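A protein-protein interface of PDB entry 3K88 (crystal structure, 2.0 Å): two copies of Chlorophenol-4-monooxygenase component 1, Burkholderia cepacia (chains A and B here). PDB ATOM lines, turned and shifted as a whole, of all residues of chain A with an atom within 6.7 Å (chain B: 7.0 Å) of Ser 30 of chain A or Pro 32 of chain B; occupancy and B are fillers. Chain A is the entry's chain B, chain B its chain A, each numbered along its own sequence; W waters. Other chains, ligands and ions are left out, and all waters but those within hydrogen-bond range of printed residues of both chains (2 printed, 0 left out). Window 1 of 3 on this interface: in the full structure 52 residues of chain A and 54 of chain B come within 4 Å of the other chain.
Of chain A, only Ser 30 (3.5 Å) comes within 4 Å of Pro 32 of chain B. Of the printed residues of chain B, His 167 of chain A touches Pro 163 (3.3 Å). Of the printed residues of chain A, Trp 86 of chain B touches Leu 26 (3.9 Å) and Ala 29 (3.6 Å). Printed residues of chain B within 4 Å of Arg 168 of chain A: Cys 161. Ser 27 of chain A touches none of the printed residues of chain B. The nearest residue of chain B that does not touch Ser 30 of chain A is Ile 165 of chain B (4.2 Å).
The guanidinium group of Arg 168 of chain A is in hydrogen-bond range of the backbone carbonyl oxygen of Cys 161 of chain B (3.1 Å).
Among the printed residues, merely in contact across the chains: Ser 30 of chain A with Pro 163 of chain B (2.8 Å), Ile 165 of chain A with Ser 30 of chain B (3.0 Å), His 167 of chain A with Pro 163 of chain B (3.3 Å), Ser 30 of chain A with Pro 32 of chain B (3.5 Å), Ala 29 of chain A with Trp 86 of chain B (3.6 Å), Pro 32 of chain A with Ser 30 of chain B (3.6 Å), Ala 29 of chain A with Val 130 of chain B (3.8 Å), Leu 26 of chain A with Trp 86 of chain B (3.9 Å), Ile 165 of chain A with Thr 174 of chain B (3.9 Å), Lys 28 of chain A with Val 130 of chain B (3.98 Å), Ser 30 of chain A with Thr 174 of chain B (3.98 Å) and Lys 28 of chain A with Pro 163 of chain B (3.99 Å).
Water W2 lies within hydrogen-bond range of O of Ala 129 of chain B (2.8 Å) and NH1 of Arg 168 of chain A (3.4 Å). Water W1 lies within hydrogen-bond range of NE1 of Trp 86 of chain B (3.0 Å) and O of Ser 30 of chain A (3.3 Å).
Ser 30 of chain A touches Pro 32 of chain B, and with the chains exchanged Pro 32 of chain A touches Ser 30 of chain B. Ile 165 of chain A touches Ser 30 of chain B, but with the chains exchanged Ser 30 of chain A does not touch Ile 165 of chain B (4.2 Å). 5 positions are printed for both chains. Of the 13 pairs that touch across the chains among the printed residues, 2 have their exchanged pair printed and touching as well.
The backbone carbonyl oxygen (O) of Trp 86 of chain B is in hydrogen-bond range of the backbone NH (N) of Ala 129 of chain B, 2.9 Å away. The backbone NH (N) of Trp 86 of chain B is in hydrogen-bond range of the backbone carbonyl oxygen (O) of Val 130 of chain B (2.8 Å). O of Ser 27 of chain A lies within hydrogen-bond range of N of Arg 168 of chain A (2.8 Å). The backbone carbonyl oxygen (O) of Lys 28 of chain A sits at hydrogen-bond distance from a ring nitrogen (NE2) of His 167 of chain A (3.2 Å).
Of the 11 printed residues of chain A, 8 touch a printed residue of chain B. Of the 21 printed residues of chain B, 7 touch a printed residue of chain A.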
ATOM      1  N   LEU A  26      31.847 -13.738 -24.551  1.00  0.00           N
ATOM      2  CA  LEU A  26      30.918 -14.844 -24.322  1.00  0.00           C
ATOM      3  C   LEU A  26      29.429 -14.414 -24.145  1.00  0.00           C
ATOM      4  O   LEU A  26      28.504 -15.206 -24.470  1.00  0.00           O
ATOM      5  CB  LEU A  26      31.374 -15.699 -23.112  1.00  0.00           C
ATOM      6  CG  LEU A  26      32.533 -16.664 -23.499  1.00  0.00           C
ATOM      7  CD1 LEU A  26      33.086 -17.346 -22.311  1.00  0.00           C
ATOM      8  CD2 LEU A  26      32.088 -17.641 -24.514  1.00  0.00           C
ATOM      9  N   SER A  27      29.167 -13.196 -23.649  1.00  0.00           N
ATOM     10  CA  SER A  27      27.759 -12.748 -23.647  1.00  0.00           C
ATOM     11  C   SER A  27      27.128 -12.795 -25.055  1.00  0.00           C
ATOM     12  O   SER A  27      25.898 -12.880 -25.203  1.00  0.00           O
ATOM     13  CB  SER A  27      27.595 -11.336 -23.017  1.00  0.00           C
ATOM     14  OG  SER A  27      28.041 -10.298 -23.912  1.00  0.00           O
ATOM     15  N   LYS A  28      27.949 -12.721 -26.100  1.00  0.00           N
ATOM     16  CA  LYS A  28      27.408 -12.735 -27.465  1.00  0.00           C
ATOM     17  C   LYS A  28      27.160 -14.157 -28.013  1.00  0.00           C
ATOM     18  O   LYS A  28      26.524 -14.334 -29.044  1.00  0.00           O
ATOM     19  CB  LYS A  28      28.343 -11.950 -28.373  1.00  0.00           C
ATOM     20  CG  LYS A  28      28.364 -10.443 -27.975  1.00  0.00           C
ATOM     21  CD  LYS A  28      29.574  -9.734 -28.641  1.00  0.00           C
ATOM     22  CE  LYS A  28      29.915  -8.385 -27.956  1.00  0.00           C
ATOM     23  NZ  LYS A  28      31.237  -7.874 -28.499  1.00  0.00           N
ATOM     24  N   ALA A  29      27.644 -15.175 -27.294  1.00  0.00           N
ATOM     25  CA  ALA A  29      27.324 -16.543 -27.673  1.00  0.00           C
ATOM     26  C   ALA A  29      25.964 -16.910 -27.167  1.00  0.00           C
ATOM     27  O   ALA A  29      25.367 -16.219 -26.317  1.00  0.00           O
ATOM     28  CB  ALA A  29      28.386 -17.552 -27.136  1.00  0.00           C
ATOM     29  N   SER A  30      25.438 -17.999 -27.706  1.00  0.00           N
ATOM     30  CA  SER A  30      24.168 -18.530 -27.246  1.00  0.00           C
ATOM     31  C   SER A  30      24.421 -19.837 -26.482  1.00  0.00           C
ATOM     32  O   SER A  30      25.315 -20.565 -26.895  1.00  0.00           O
ATOM     33  CB  SER A  30      23.334 -18.811 -28.430  1.00  0.00           C
ATOM     34  OG  SER A  30      22.677 -17.580 -28.770  1.00  0.00           O
ATOM     35  N   THR A  31      23.692 -20.113 -25.391  1.00  0.00           N
ATOM     36  CA  THR A  31      23.738 -21.455 -24.726  1.00  0.00           C
ATOM     37  C   THR A  31      22.323 -22.012 -24.367  1.00  0.00           C
ATOM     38  O   THR A  31      21.399 -21.248 -24.166  1.00  0.00           O
ATOM     39  CB  THR A  31      24.466 -21.356 -23.391  1.00  0.00           C
ATOM     40  OG1 THR A  31      23.766 -20.421 -22.564  1.00  0.00           O
ATOM     41  CG2 THR A  31      25.908 -20.874 -23.553  1.00  0.00           C
ATOM     42  N   PRO A  32      22.169 -23.339 -24.223  1.00  0.00           N
ATOM     43  CA  PRO A  32      20.960 -23.827 -23.573  1.00  0.00           C
ATOM     44  C   PRO A  32      21.029 -23.454 -22.095  1.00  0.00           C
ATOM     45  O   PRO A  32      22.053 -22.960 -21.651  1.00  0.00           O
ATOM     46  CB  PRO A  32      21.113 -25.326 -23.694  1.00  0.00           C
ATOM     47  CG  PRO A  32      22.638 -25.488 -23.587  1.00  0.00           C
ATOM     48  CD  PRO A  32      23.051 -24.457 -24.582  1.00  0.00           C
ATOM     49  N   ILE A 165      16.850 -20.727 -24.232  1.00  0.00           N
ATOM     50  CA  ILE A 165      18.197 -20.365 -24.671  1.00  0.00           C
ATOM     51  C   ILE A 165      18.601 -19.078 -23.869  1.00  0.00           C
ATOM     52  O   ILE A 165      17.716 -18.318 -23.427  1.00  0.00           O
ATOM     53  CB  ILE A 165      18.145 -20.065 -26.181  1.00  0.00           C
ATOM     54  CG1 ILE A 165      17.641 -21.280 -26.968  1.00  0.00           C
ATOM     55  CG2 ILE A 165      19.442 -19.531 -26.708  1.00  0.00           C
ATOM     56  CD1 ILE A 165      18.599 -22.444 -27.034  1.00  0.00           C
ATOM     57  N   TYR A 166      19.900 -18.830 -23.686  1.00  0.00           N
ATOM     58  CA  TYR A 166      20.362 -17.631 -22.995  1.00  0.00           C
ATOM     59  C   TYR A 166      21.348 -16.968 -23.915  1.00  0.00           C
ATOM     60  O   TYR A 166      22.281 -17.629 -24.455  1.00  0.00           O
ATOM     61  CB  TYR A 166      21.054 -17.981 -21.670  1.00  0.00           C
ATOM     62  CG  TYR A 166      21.178 -16.833 -20.710  1.00  0.00           C
ATOM     63  CD1 TYR A 166      20.050 -16.238 -20.146  1.00  0.00           C
ATOM     64  CD2 TYR A 166      22.432 -16.334 -20.360  1.00  0.00           C
ATOM     65  CE1 TYR A 166      20.169 -15.153 -19.230  1.00  0.00           C
ATOM     66  CE2 TYR A 166      22.565 -15.284 -19.441  1.00  0.00           C
ATOM     67  CZ  TYR A 166      21.420 -14.690 -18.891  1.00  0.00           C
ATOM     68  OH  TYR A 166      21.598 -13.649 -17.988  1.00  0.00           O
ATOM     69  N   HIS A 167      21.159 -15.668 -24.107  1.00  0.00           N
ATOM     70  CA  HIS A 167      21.923 -14.979 -25.140  1.00  0.00           C
ATOM     71  C   HIS A 167      21.946 -13.485 -24.848  1.00  0.00           C
ATOM     72  O   HIS A 167      20.903 -12.920 -24.575  1.00  0.00           O
ATOM     73  CB  HIS A 167      21.292 -15.224 -26.515  1.00  0.00           C
ATOM     74  CG  HIS A 167      21.988 -14.471 -27.599  1.00  0.00           C
ATOM     75  ND1 HIS A 167      21.356 -13.540 -28.393  1.00  0.00           N
ATOM     76  CD2 HIS A 167      23.294 -14.451 -27.961  1.00  0.00           C
ATOM     77  CE1 HIS A 167      22.232 -13.014 -29.236  1.00  0.00           C
ATOM     78  NE2 HIS A 167      23.415 -13.548 -28.989  1.00  0.00           N
ATOM     79  N   ARG A 168      23.132 -12.876 -24.833  1.00  0.00           N
ATOM     80  CA  ARG A 168      23.281 -11.451 -24.442  1.00  0.00           C
ATOM     81  C   ARG A 168      22.471 -11.194 -23.230  1.00  0.00           C
ATOM     82  O   ARG A 168      21.647 -10.326 -23.245  1.00  0.00           O
ATOM     83  CB  ARG A 168      22.853 -10.464 -25.540  1.00  0.00           C
ATOM     84  CG  ARG A 168      23.513 -10.740 -26.860  1.00  0.00           C
ATOM     85  CD  ARG A 168      23.528  -9.602 -27.907  1.00  0.00           C
ATOM     86  NE  ARG A 168      24.684  -9.858 -28.801  1.00  0.00           N
ATOM     87  CZ  ARG A 168      24.645 -10.291 -30.079  1.00  0.00           C
ATOM     88  NH1 ARG A 168      25.804 -10.509 -30.750  1.00  0.00           N
ATOM     89  NH2 ARG A 168      23.458 -10.482 -30.701  1.00  0.00           N
ATOM     90  N   SER B  30      19.443 -28.395 -27.119  1.00  0.00           N
ATOM     91  CA  SER B  30      19.970 -27.489 -28.142  1.00  0.00           C
ATOM     92  C   SER B  30      21.422 -27.153 -27.783  1.00  0.00           C
ATOM     93  O   SER B  30      21.796 -27.287 -26.606  1.00  0.00           O
ATOM     94  CB  SER B  30      19.084 -26.228 -28.306  1.00  0.00           C
ATOM     95  OG  SER B  30      19.204 -25.376 -27.185  1.00  0.00           O
ATOM     96  N   THR B  31      22.226 -26.765 -28.782  1.00  0.00           N
ATOM     97  CA  THR B  31      23.612 -26.372 -28.588  1.00  0.00           C
ATOM     98  C   THR B  31      23.978 -25.196 -29.483  1.00  0.00           C
ATOM     99  O   THR B  31      23.360 -24.963 -30.497  1.00  0.00           O
ATOM    100  CB  THR B  31      24.607 -27.505 -29.053  1.00  0.00           C
ATOM    101  OG1 THR B  31      24.387 -27.840 -30.450  1.00  0.00           O
ATOM    102  CG2 THR B  31      24.474 -28.745 -28.181  1.00  0.00           C
ATOM    103  N   PRO B  32      25.051 -24.495 -29.153  1.00  0.00           N
ATOM    104  CA  PRO B  32      25.599 -23.546 -30.125  1.00  0.00           C
ATOM    105  C   PRO B  32      26.341 -24.353 -31.182  1.00  0.00           C
ATOM    106  O   PRO B  32      26.480 -25.591 -31.078  1.00  0.00           O
ATOM    107  CB  PRO B  32      26.639 -22.796 -29.308  1.00  0.00           C
ATOM    108  CG  PRO B  32      27.035 -23.784 -28.239  1.00  0.00           C
ATOM    109  CD  PRO B  32      25.740 -24.423 -27.856  1.00  0.00           C
ATOM    110  N   VAL B  33      26.759 -23.674 -32.233  1.00  0.00           N
ATOM    111  CA  VAL B  33      27.493 -24.339 -33.297  1.00  0.00           C
ATOM    112  C   VAL B  33      28.784 -23.588 -33.455  1.00  0.00           C
ATOM    113  O   VAL B  33      28.745 -22.408 -33.699  1.00  0.00           O
ATOM    114  CB  VAL B  33      26.702 -24.392 -34.631  1.00  0.00           C
ATOM    115  CG1 VAL B  33      27.466 -25.233 -35.651  1.00  0.00           C
ATOM    116  CG2 VAL B  33      25.343 -25.031 -34.401  1.00  0.00           C
ATOM    117  N   THR B  34      29.931 -24.258 -33.280  1.00  0.00           N
ATOM    118  CA  THR B  34      31.232 -23.593 -33.511  1.00  0.00           C
ATOM    119  C   THR B  34      32.031 -24.268 -34.620  1.00  0.00           C
ATOM    120  O   THR B  34      31.753 -25.444 -34.998  1.00  0.00           O
ATOM    121  CB  THR B  34      32.109 -23.555 -32.240  1.00  0.00           C
ATOM    122  OG1 THR B  34      32.767 -24.815 -32.070  1.00  0.00           O
ATOM    123  CG2 THR B  34      31.253 -23.287 -30.977  1.00  0.00           C
ATOM    124  N   CYS B  49      32.023 -28.155 -34.177  1.00  0.00           N
ATOM    125  CA  CYS B  49      32.034 -28.695 -32.818  1.00  0.00           C
ATOM    126  C   CYS B  49      30.919 -27.982 -32.038  1.00  0.00           C
ATOM    127  O   CYS B  49      30.765 -26.751 -32.093  1.00  0.00           O
ATOM    128  CB  CYS B  49      33.458 -28.566 -32.225  1.00  0.00           C
ATOM    129  SG  CYS B  49      33.539 -28.891 -30.379  1.00  0.00           S
ATOM    130  N   SER B  50      30.036 -28.745 -31.440  1.00  0.00           N
ATOM    131  CA  SER B  50      28.991 -28.147 -30.613  1.00  0.00           C
ATOM    132  C   SER B  50      29.293 -28.393 -29.119  1.00  0.00           C
ATOM    133  O   SER B  50      28.709 -27.753 -28.270  1.00  0.00           O
ATOM    134  CB  SER B  50      27.607 -28.670 -30.987  1.00  0.00           C
ATOM    135  OG  SER B  50      27.535 -30.096 -30.823  1.00  0.00           O
ATOM    136  N   ALA B  51      30.227 -29.286 -28.798  1.00  0.00           N
ATOM    137  CA  ALA B  51      30.432 -29.666 -27.383  1.00  0.00           C
ATOM    138  C   ALA B  51      31.540 -28.766 -26.845  1.00  0.00           C
ATOM    139  O   ALA B  51      32.717 -29.138 -26.735  1.00  0.00           O
ATOM    140  CB  ALA B  51      30.779 -31.235 -27.255  1.00  0.00           C
ATOM    141  N   VAL B  52      31.173 -27.524 -26.622  1.00  0.00           N
ATOM    142  CA  VAL B  52      32.117 -26.487 -26.272  1.00  0.00           C
ATOM    143  C   VAL B  52      31.525 -25.797 -25.061  1.00  0.00           C
ATOM    144  O   VAL B  52      30.298 -25.604 -24.993  1.00  0.00           O
ATOM    145  CB  VAL B  52      32.215 -25.441 -27.438  1.00  0.00           C
ATOM    146  CG1 VAL B  52      33.079 -24.292 -27.019  1.00  0.00           C
ATOM    147  CG2 VAL B  52      32.853 -26.037 -28.668  1.00  0.00           C
ATOM    148  N   CYS B  53      32.337 -25.427 -24.095  1.00  0.00           N
ATOM    149  CA  CYS B  53      31.786 -24.501 -23.103  1.00  0.00           C
ATOM    150  C   CYS B  53      32.818 -23.705 -22.355  1.00  0.00           C
ATOM    151  O   CYS B  53      34.035 -23.991 -22.463  1.00  0.00           O
ATOM    152  CB  CYS B  53      30.824 -25.192 -22.131  1.00  0.00           C
ATOM    153  SG  CYS B  53      31.648 -26.183 -20.983  1.00  0.00           S
ATOM    154  N   TRP B  86      32.264 -19.290 -32.730  1.00  0.00           N
ATOM    155  CA  TRP B  86      30.814 -19.441 -32.606  1.00  0.00           C
ATOM    156  C   TRP B  86      30.111 -18.818 -33.791  1.00  0.00           C
ATOM    157  O   TRP B  86      30.218 -17.631 -34.015  1.00  0.00           O
ATOM    158  CB  TRP B  86      30.326 -18.752 -31.322  1.00  0.00           C
ATOM    159  CG  TRP B  86      30.614 -19.427 -29.999  1.00  0.00           C
ATOM    160  CD1 TRP B  86      29.701 -20.107 -29.253  1.00  0.00           C
ATOM    161  CD2 TRP B  86      31.858 -19.478 -29.252  1.00  0.00           C
ATOM    162  NE1 TRP B  86      30.274 -20.573 -28.113  1.00  0.00           N
ATOM    163  CE2 TRP B  86      31.595 -20.227 -28.081  1.00  0.00           C
ATOM    164  CE3 TRP B  86      33.148 -18.993 -29.468  1.00  0.00           C
ATOM    165  CZ2 TRP B  86      32.545 -20.458 -27.102  1.00  0.00           C
ATOM    166  CZ3 TRP B  86      34.122 -19.234 -28.518  1.00  0.00           C
ATOM    167  CH2 TRP B  86      33.806 -19.973 -27.320  1.00  0.00           C
ATOM    168  N   LEU B  87      29.381 -19.627 -34.547  1.00  0.00           N
ATOM    169  CA  LEU B  87      28.890 -19.205 -35.833  1.00  0.00           C
ATOM    170  C   LEU B  87      27.612 -18.354 -35.675  1.00  0.00           C
ATOM    171  O   LEU B  87      26.842 -18.584 -34.762  1.00  0.00           O
ATOM    172  CB  LEU B  87      28.538 -20.459 -36.612  1.00  0.00           C
ATOM    173  CG  LEU B  87      29.538 -20.917 -37.683  1.00  0.00           C
ATOM    174  CD1 LEU B  87      31.016 -20.422 -37.585  1.00  0.00           C
ATOM    175  CD2 LEU B  87      29.396 -22.393 -37.955  1.00  0.00           C
ATOM    176  N   ALA B 129      30.011 -14.813 -34.652  1.00  0.00           N
ATOM    177  CA  ALA B 129      29.479 -14.075 -33.497  1.00  0.00           C
ATOM    178  C   ALA B 129      30.536 -13.906 -32.381  1.00  0.00           C
ATOM    179  O   ALA B 129      30.504 -12.915 -31.666  1.00  0.00           O
ATOM    180  CB  ALA B 129      28.222 -14.721 -32.976  1.00  0.00           C
ATOM    181  N   VAL B 130      31.456 -14.873 -32.231  1.00  0.00           N
ATOM    182  CA  VAL B 130      32.544 -14.843 -31.240  1.00  0.00           C
ATOM    183  C   VAL B 130      33.681 -15.664 -31.778  1.00  0.00           C
ATOM    184  O   VAL B 130      33.483 -16.773 -32.279  1.00  0.00           O
ATOM    185  CB  VAL B 130      32.157 -15.488 -29.860  1.00  0.00           C
ATOM    186  CG1 VAL B 130      33.271 -15.261 -28.792  1.00  0.00           C
ATOM    187  CG2 VAL B 130      30.835 -14.924 -29.323  1.00  0.00           C
ATOM    188  N   CYS B 161      25.564 -10.092 -34.039  1.00  0.00           N
ATOM    189  CA  CYS B 161      25.323 -11.376 -34.680  1.00  0.00           C
ATOM    190  C   CYS B 161      24.408 -12.250 -33.814  1.00  0.00           C
ATOM    191  O   CYS B 161      24.780 -12.688 -32.713  1.00  0.00           O
ATOM    192  CB  CYS B 161      26.636 -12.161 -34.897  1.00  0.00           C
ATOM    193  SG  CYS B 161      27.755 -11.639 -36.203  1.00  0.00           S
ATOM    194  N   THR B 162      23.232 -12.525 -34.351  1.00  0.00           N
ATOM    195  CA  THR B 162      22.326 -13.550 -33.878  1.00  0.00           C
ATOM    196  C   THR B 162      22.872 -15.008 -34.144  1.00  0.00           C
ATOM    197  O   THR B 162      23.338 -15.337 -35.214  1.00  0.00           O
ATOM    198  CB  THR B 162      20.954 -13.198 -34.519  1.00  0.00           C
ATOM    199  OG1 THR B 162      20.219 -12.315 -33.637  1.00  0.00           O
ATOM    200  CG2 THR B 162      20.149 -14.389 -34.840  1.00  0.00           C
ATOM    201  N   PRO B 163      22.872 -15.875 -33.136  1.00  0.00           N
ATOM    202  CA  PRO B 163      23.779 -17.021 -33.297  1.00  0.00           C
ATOM    203  C   PRO B 163      23.142 -18.225 -33.992  1.00  0.00           C
ATOM    204  O   PRO B 163      21.918 -18.351 -34.091  1.00  0.00           O
ATOM    205  CB  PRO B 163      24.176 -17.370 -31.842  1.00  0.00           C
ATOM    206  CG  PRO B 163      23.588 -16.216 -30.985  1.00  0.00           C
ATOM    207  CD  PRO B 163      22.366 -15.769 -31.768  1.00  0.00           C
ATOM    208  N   LEU B 164      23.987 -19.121 -34.476  1.00  0.00           N
ATOM    209  CA  LEU B 164      23.514 -20.340 -35.062  1.00  0.00           C
ATOM    210  C   LEU B 164      23.349 -21.358 -33.944  1.00  0.00           C
ATOM    211  O   LEU B 164      24.232 -21.493 -33.104  1.00  0.00           O
ATOM    212  CB  LEU B 164      24.527 -20.830 -36.106  1.00  0.00           C
ATOM    213  CG  LEU B 164      24.156 -22.060 -36.913  1.00  0.00           C
ATOM    214  CD1 LEU B 164      22.915 -21.756 -37.723  1.00  0.00           C
ATOM    215  CD2 LEU B 164      25.317 -22.430 -37.873  1.00  0.00           C
ATOM    216  N   ILE B 165      22.214 -22.059 -33.937  1.00  0.00           N
ATOM    217  CA  ILE B 165      21.892 -23.035 -32.917  1.00  0.00           C
ATOM    218  C   ILE B 165      21.617 -24.364 -33.615  1.00  0.00           C
ATOM    219  O   ILE B 165      21.275 -24.363 -34.783  1.00  0.00           O
ATOM    220  CB  ILE B 165      20.676 -22.550 -32.068  1.00  0.00           C
ATOM    221  CG1 ILE B 165      21.192 -21.563 -31.015  1.00  0.00           C
ATOM    222  CG2 ILE B 165      19.957 -23.724 -31.374  1.00  0.00           C
ATOM    223  CD1 ILE B 165      20.200 -20.575 -30.687  1.00  0.00           C
ATOM    224  N   TYR B 166      21.852 -25.487 -32.936  1.00  0.00           N
ATOM    225  CA  TYR B 166      21.446 -26.802 -33.480  1.00  0.00           C
ATOM    226  C   TYR B 166      20.486 -27.442 -32.449  1.00  0.00           C
ATOM    227  O   TYR B 166      20.798 -27.465 -31.245  1.00  0.00           O
ATOM    228  CB  TYR B 166      22.666 -27.718 -33.652  1.00  0.00           C
ATOM    229  CG  TYR B 166      22.522 -28.871 -34.635  1.00  0.00           C
ATOM    230  CD1 TYR B 166      22.470 -28.643 -35.991  1.00  0.00           C
ATOM    231  CD2 TYR B 166      22.545 -30.190 -34.195  1.00  0.00           C
ATOM    232  CE1 TYR B 166      22.387 -29.705 -36.920  1.00  0.00           C
ATOM    233  CE2 TYR B 166      22.466 -31.249 -35.102  1.00  0.00           C
ATOM    234  CZ  TYR B 166      22.373 -30.988 -36.463  1.00  0.00           C
ATOM    235  OH  TYR B 166      22.307 -32.065 -37.313  1.00  0.00           O
ATOM    236  N   THR B 174      17.838 -17.662 -32.828  1.00  0.00           N
ATOM    237  CA  THR B 174      17.044 -17.270 -31.661  1.00  0.00           C
ATOM    238  C   THR B 174      15.885 -16.316 -31.993  1.00  0.00           C
ATOM    239  O   THR B 174      15.905 -15.607 -33.017  1.00  0.00           O
ATOM    240  CB  THR B 174      17.935 -16.614 -30.576  1.00  0.00           C
ATOM    241  OG1 THR B 174      18.712 -15.563 -31.156  1.00  0.00           O
ATOM    242  CG2 THR B 174      18.900 -17.613 -30.015  1.00  0.00           C
HETATM  243  O   HOH W   1      28.388 -21.392 -25.950  1.00  0.00           O
HETATM  244  O   HOH W   2      28.991 -10.573 -31.917  1.00  0.00           O
